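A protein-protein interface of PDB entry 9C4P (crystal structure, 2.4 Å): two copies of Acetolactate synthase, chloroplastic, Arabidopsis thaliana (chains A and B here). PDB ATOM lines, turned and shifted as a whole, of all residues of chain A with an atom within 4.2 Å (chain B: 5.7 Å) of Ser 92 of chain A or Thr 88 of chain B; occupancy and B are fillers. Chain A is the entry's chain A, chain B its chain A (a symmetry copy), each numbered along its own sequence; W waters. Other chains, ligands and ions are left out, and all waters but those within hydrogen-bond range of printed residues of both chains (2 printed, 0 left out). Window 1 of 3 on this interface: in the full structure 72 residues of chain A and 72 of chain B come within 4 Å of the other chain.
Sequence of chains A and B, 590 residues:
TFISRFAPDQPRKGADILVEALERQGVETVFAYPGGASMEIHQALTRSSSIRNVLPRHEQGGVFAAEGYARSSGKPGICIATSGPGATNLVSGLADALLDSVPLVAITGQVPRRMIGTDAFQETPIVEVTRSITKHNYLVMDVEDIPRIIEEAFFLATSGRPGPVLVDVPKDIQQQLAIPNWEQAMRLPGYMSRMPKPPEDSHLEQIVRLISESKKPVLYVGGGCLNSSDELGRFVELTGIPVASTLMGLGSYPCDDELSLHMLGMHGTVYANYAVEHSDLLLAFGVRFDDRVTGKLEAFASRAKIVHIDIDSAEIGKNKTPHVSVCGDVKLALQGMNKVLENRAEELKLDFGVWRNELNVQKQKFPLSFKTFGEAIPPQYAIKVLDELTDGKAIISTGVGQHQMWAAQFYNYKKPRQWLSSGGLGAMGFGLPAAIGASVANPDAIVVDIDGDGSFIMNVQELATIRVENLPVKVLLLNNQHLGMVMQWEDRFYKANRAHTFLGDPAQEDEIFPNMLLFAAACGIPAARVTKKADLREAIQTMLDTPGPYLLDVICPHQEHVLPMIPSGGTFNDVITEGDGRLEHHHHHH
Of chain A, only Val 91 and Ser 92 come within 4 Å of Thr 88 of chain B. Printed residues of chain A within 4 Å of Thr 124 of chain B: Leu 425. Of the printed residues of chain A, Asn 89 of chain B touches Gln 60 (2.8 Å) and Ser 92 (2.9 Å). Of the printed residues of chain B, Leu 425 of chain A touches Gly 84, Pro 85 and Thr 124. Printed residues of chain A within 4 Å of Pro 85 of chain B: Leu 425 (3.2 Å). Ala 95 of chain A touches none of the printed residues of chain B. The nearest printed residue of chain A that does not touch Thr 88 of chain B is Ala 95 of chain A (4.4 Å). The nearest printed residue of chain B that does not touch Gln 60 of chain A is Thr 88 of chain B (6.1 Å).
The backbone carbonyl oxygen (O) of Gly 84 of chain B lies within hydrogen-bond range of the side-chain hydroxyl (OG1) of Thr 88 of chain B, 3.3 Å away. O of Pro 85 of chain B sits at hydrogen-bond distance from OG1 of Thr 88 of chain B (3.3 Å). The backbone carbonyl oxygen (O) of Pro 85 of chain B sits close to the side-chain amide nitrogen (ND2) of Asn 89 of chain B (3.3 Å).
Of the 9 printed residues of chain A, 4 touch a printed residue of chain B. Hydrophobic or aromatic side chains of chain B that line the printed part of chain A: Pro 85.
Positions printed for both chains: 90, 91 and 92. Of the 7 pairs that touch across the chains among the printed residues, none has its exchanged pair printed and touching as well.
Water W1 lies within hydrogen-bond range of O of Pro 85 of chain B, OG of Ser 92 of chain A and OD1 of Asn 89 of chain B. Water W2 bridges OE1 of Gln 60 of chain A (3.0 Å) and ND2 of Asn 89 of chain B (3.0 Å).
CG1 of Val 91 of chain A touches CB of Thr 88 of chain B (3.9 Å). Gly 84 of chain B touches Leu 425 of chain A (CA to CD1, 3.6 Å). CD of Pro 85 of chain B touches O of Leu 425 of chain A, 3.2 Å away. Leu 425 of chain A touches Thr 124 of chain B (CD1 to OG1, 3.5 Å).
OG of Ser 92 of chain A sits at hydrogen-bond distance from OD1 of Asn 89 of chain B, 2.9 Å away. NE2 of Gln 60 of chain A is in hydrogen-bond range of OD1 of Asn 89 of chain B, at 2.8 Å. The side-chain hydroxyl (OG1) of Thr 88 of chain B is in hydrogen-bond range of the side-chain hydroxyl (OG) of Ser 92 of chain A (2.6 Å).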
ATOM      1  N   GLN A  60       9.387  22.269 -36.373  1.00  0.00           N
ATOM      2  CA  GLN A  60      10.109  23.049 -35.373  1.00  0.00           C
ATOM      3  C   GLN A  60      10.565  24.379 -35.957  1.00  0.00           C
ATOM      4  O   GLN A  60      10.549  25.408 -35.271  1.00  0.00           O
ATOM      5  CB  GLN A  60      11.302  22.266 -34.826  1.00  0.00           C
ATOM      6  CG  GLN A  60      12.145  23.090 -33.856  1.00  0.00           C
ATOM      7  CD  GLN A  60      13.202  22.282 -33.136  1.00  0.00           C
ATOM      8  OE1 GLN A  60      14.395  22.425 -33.404  1.00  0.00           O
ATOM      9  NE2 GLN A  60      12.773  21.440 -32.199  1.00  0.00           N
ATOM     10  N   LEU A  90       6.264  20.328 -32.950  1.00  0.00           N
ATOM     11  CA  LEU A  90       6.006  21.669 -32.435  1.00  0.00           C
ATOM     12  C   LEU A  90       6.415  21.837 -30.980  1.00  0.00           C
ATOM     13  O   LEU A  90       6.459  22.974 -30.498  1.00  0.00           O
ATOM     14  CB  LEU A  90       4.519  22.009 -32.548  1.00  0.00           C
ATOM     15  CG  LEU A  90       3.863  22.106 -33.920  1.00  0.00           C
ATOM     16  CD1 LEU A  90       2.383  22.382 -33.738  1.00  0.00           C
ATOM     17  CD2 LEU A  90       4.519  23.202 -34.743  1.00  0.00           C
ATOM     18  N   VAL A  91       6.727  20.741 -30.286  1.00  0.00           N
ATOM     19  CA  VAL A  91       6.707  20.730 -28.824  1.00  0.00           C
ATOM     20  C   VAL A  91       7.768  21.664 -28.246  1.00  0.00           C
ATOM     21  O   VAL A  91       7.505  22.396 -27.282  1.00  0.00           O
ATOM     22  CB  VAL A  91       6.863  19.285 -28.316  1.00  0.00           C
ATOM     23  CG1 VAL A  91       7.354  19.259 -26.885  1.00  0.00           C
ATOM     24  CG2 VAL A  91       5.530  18.551 -28.437  1.00  0.00           C
ATOM     25  N   SER A  92       8.974  21.663 -28.818  1.00  0.00           N
ATOM     26  CA  SER A  92      10.027  22.537 -28.304  1.00  0.00           C
ATOM     27  C   SER A  92       9.632  24.004 -28.415  1.00  0.00           C
ATOM     28  O   SER A  92       9.937  24.806 -27.524  1.00  0.00           O
ATOM     29  CB  SER A  92      11.342  22.281 -29.039  1.00  0.00           C
ATOM     30  OG  SER A  92      11.865  21.006 -28.717  1.00  0.00           O
ATOM     31  N   GLY A  93       8.946  24.375 -29.497  1.00  0.00           N
ATOM     32  CA  GLY A  93       8.537  25.760 -29.660  1.00  0.00           C
ATOM     33  C   GLY A  93       7.409  26.155 -28.725  1.00  0.00           C
ATOM     34  O   GLY A  93       7.350  27.298 -28.260  1.00  0.00           O
ATOM     35  N   LEU A  94       6.496  25.224 -28.445  1.00  0.00           N
ATOM     36  CA  LEU A  94       5.440  25.492 -27.474  1.00  0.00           C
ATOM     37  C   LEU A  94       6.030  25.761 -26.096  1.00  0.00           C
ATOM     38  O   LEU A  94       5.716  26.774 -25.457  1.00  0.00           O
ATOM     39  CB  LEU A  94       4.461  24.318 -27.426  1.00  0.00           C
ATOM     40  CG  LEU A  94       3.738  23.999 -28.734  1.00  0.00           C
ATOM     41  CD1 LEU A  94       2.864  22.767 -28.577  1.00  0.00           C
ATOM     42  CD2 LEU A  94       2.913  25.193 -29.185  1.00  0.00           C
ATOM     43  N   ALA A  95       6.894  24.859 -25.621  1.00  0.00           N
ATOM     44  CA  ALA A  95       7.555  25.068 -24.338  1.00  0.00           C
ATOM     45  C   ALA A  95       8.368  26.356 -24.344  1.00  0.00           C
ATOM     46  O   ALA A  95       8.394  27.087 -23.346  1.00  0.00           O
ATOM     47  CB  ALA A  95       8.448  23.874 -24.008  1.00  0.00           C
ATOM     48  N   ASP A  96       9.035  26.649 -25.461  1.00  0.00           N
ATOM     49  CA  ASP A  96       9.827  27.872 -25.561  1.00  0.00           C
ATOM     50  C   ASP A  96       8.944  29.106 -25.419  1.00  0.00           C
ATOM     51  O   ASP A  96       9.282  30.046 -24.690  1.00  0.00           O
ATOM     52  CB  ASP A  96      10.581  27.888 -26.893  1.00  0.00           C
ATOM     53  CG  ASP A  96      11.667  28.941 -26.938  1.00  0.00           C
ATOM     54  OD1 ASP A  96      12.466  29.016 -25.982  1.00  0.00           O
ATOM     55  OD2 ASP A  96      11.733  29.685 -27.940  1.00  0.00           O
ATOM     56  N   LEU A 425      13.739  28.658 -21.846  1.00  0.00           N
ATOM     57  CA  LEU A 425      14.077  27.304 -22.269  1.00  0.00           C
ATOM     58  C   LEU A 425      15.491  27.239 -22.838  1.00  0.00           C
ATOM     59  O   LEU A 425      16.211  26.260 -22.611  1.00  0.00           O
ATOM     60  CB  LEU A 425      13.058  26.814 -23.301  1.00  0.00           C
ATOM     61  CG  LEU A 425      13.131  25.356 -23.753  1.00  0.00           C
ATOM     62  CD1 LEU A 425      12.691  24.422 -22.638  1.00  0.00           C
ATOM     63  CD2 LEU A 425      12.288  25.136 -25.005  1.00  0.00           C
ATOM     64  N   GLY B  84      15.061  20.454 -20.577  1.00  0.00           N
ATOM     65  CA  GLY B  84      14.407  21.473 -21.363  1.00  0.00           C
ATOM     66  C   GLY B  84      14.394  21.203 -22.855  1.00  0.00           C
ATOM     67  O   GLY B  84      13.770  20.249 -23.335  1.00  0.00           O
ATOM     68  N   PRO B  85      15.096  22.048 -23.619  1.00  0.00           N
ATOM     69  CA  PRO B  85      15.052  21.923 -25.086  1.00  0.00           C
ATOM     70  C   PRO B  85      15.684  20.649 -25.606  1.00  0.00           C
ATOM     71  O   PRO B  85      15.329  20.205 -26.706  1.00  0.00           O
ATOM     72  CB  PRO B  85      15.823  23.160 -25.562  1.00  0.00           C
ATOM     73  CG  PRO B  85      16.789  23.428 -24.455  1.00  0.00           C
ATOM     74  CD  PRO B  85      16.049  23.082 -23.181  1.00  0.00           C
ATOM     75  N   GLY B  86      16.621  20.054 -24.868  1.00  0.00           N
ATOM     76  CA  GLY B  86      17.112  18.744 -25.256  1.00  0.00           C
ATOM     77  C   GLY B  86      16.040  17.683 -25.104  1.00  0.00           C
ATOM     78  O   GLY B  86      15.810  16.879 -26.011  1.00  0.00           O
ATOM     79  N   ALA B  87      15.348  17.693 -23.960  1.00  0.00           N
ATOM     80  CA  ALA B  87      14.319  16.693 -23.695  1.00  0.00           C
ATOM     81  C   ALA B  87      13.165  16.807 -24.683  1.00  0.00           C
ATOM     82  O   ALA B  87      12.682  15.798 -25.203  1.00  0.00           O
ATOM     83  CB  ALA B  87      13.814  16.831 -22.258  1.00  0.00           C
ATOM     84  N   THR B  88      12.704  18.034 -24.955  1.00  0.00           N
ATOM     85  CA  THR B  88      11.564  18.187 -25.855  1.00  0.00           C
ATOM     86  C   THR B  88      11.911  17.775 -27.279  1.00  0.00           C
ATOM     87  O   THR B  88      11.016  17.394 -28.043  1.00  0.00           O
ATOM     88  CB  THR B  88      11.040  19.628 -25.832  1.00  0.00           C
ATOM     89  OG1 THR B  88      12.092  20.542 -26.168  1.00  0.00           O
ATOM     90  CG2 THR B  88      10.475  19.977 -24.460  1.00  0.00           C
ATOM     91  N   ASN B  89      13.191  17.830 -27.655  1.00  0.00           N
ATOM     92  CA  ASN B  89      13.606  17.360 -28.973  1.00  0.00           C
ATOM     93  C   ASN B  89      13.557  15.842 -29.109  1.00  0.00           C
ATOM     94  O   ASN B  89      13.706  15.336 -30.225  1.00  0.00           O
ATOM     95  CB  ASN B  89      15.018  17.853 -29.293  1.00  0.00           C
ATOM     96  CG  ASN B  89      15.035  19.267 -29.844  1.00  0.00           C
ATOM     97  OD1 ASN B  89      14.005  19.802 -30.253  1.00  0.00           O
ATOM     98  ND2 ASN B  89      16.216  19.871 -29.879  1.00  0.00           N
ATOM     99  N   LEU B  90      13.364  15.108 -28.012  1.00  0.00           N
ATOM    100  CA  LEU B  90      13.225  13.656 -28.071  1.00  0.00           C
ATOM    101  C   LEU B  90      11.803  13.206 -28.367  1.00  0.00           C
ATOM    102  O   LEU B  90      11.598  12.025 -28.665  1.00  0.00           O
ATOM    103  CB  LEU B  90      13.653  13.022 -26.747  1.00  0.00           C
ATOM    104  CG  LEU B  90      15.098  13.144 -26.276  1.00  0.00           C
ATOM    105  CD1 LEU B  90      15.228  12.492 -24.913  1.00  0.00           C
ATOM    106  CD2 LEU B  90      16.036  12.491 -27.278  1.00  0.00           C
ATOM    107  N   VAL B  91      10.832  14.119 -28.306  1.00  0.00           N
ATOM    108  CA  VAL B  91       9.431  13.736 -28.143  1.00  0.00           C
ATOM    109  C   VAL B  91       8.922  12.954 -29.351  1.00  0.00           C
ATOM    110  O   VAL B  91       8.210  11.952 -29.201  1.00  0.00           O
ATOM    111  CB  VAL B  91       8.581  14.988 -27.857  1.00  0.00           C
ATOM    112  CG1 VAL B  91       7.124  14.746 -28.182  1.00  0.00           C
ATOM    113  CG2 VAL B  91       8.743  15.397 -26.395  1.00  0.00           C
ATOM    114  N   SER B  92       9.275  13.389 -30.564  1.00  0.00           N
ATOM    115  CA  SER B  92       8.815  12.679 -31.755  1.00  0.00           C
ATOM    116  C   SER B  92       9.327  11.245 -31.779  1.00  0.00           C
ATOM    117  O   SER B  92       8.610  10.328 -32.198  1.00  0.00           O
ATOM    118  CB  SER B  92       9.247  13.421 -33.021  1.00  0.00           C
ATOM    119  OG  SER B  92       8.557  14.650 -33.151  1.00  0.00           O
ATOM    120  N   THR B 124      11.723  21.603 -18.056  1.00  0.00           N
ATOM    121  CA  THR B 124      10.546  21.126 -18.740  1.00  0.00           C
ATOM    122  C   THR B 124      10.033  19.967 -17.894  1.00  0.00           C
ATOM    123  O   THR B 124      10.829  19.095 -17.500  1.00  0.00           O
ATOM    124  CB  THR B 124      10.837  20.672 -20.174  1.00  0.00           C
ATOM    125  OG1 THR B 124      11.107  21.815 -20.991  1.00  0.00           O
ATOM    126  CG2 THR B 124       9.657  19.908 -20.753  1.00  0.00           C
ATOM    127  N   ILE B 126       9.192  17.000 -18.192  1.00  0.00           N
ATOM    128  CA  ILE B 126       9.227  16.036 -19.287  1.00  0.00           C
ATOM    129  C   ILE B 126       8.501  14.750 -18.915  1.00  0.00           C
ATOM    130  O   ILE B 126       7.943  14.071 -19.786  1.00  0.00           O
ATOM    131  CB  ILE B 126      10.684  15.772 -19.715  1.00  0.00           C
ATOM    132  CG1 ILE B 126      10.718  15.056 -21.064  1.00  0.00           C
ATOM    133  CG2 ILE B 126      11.439  14.975 -18.659  1.00  0.00           C
ATOM    134  CD1 ILE B 126      10.168  15.896 -22.202  1.00  0.00           C
HETATM  135  O   HOH W   1      14.638  22.286 -28.575  1.00  0.00           O
HETATM  136  O   HOH W   2      15.954  22.670 -30.903  1.00  0.00           O
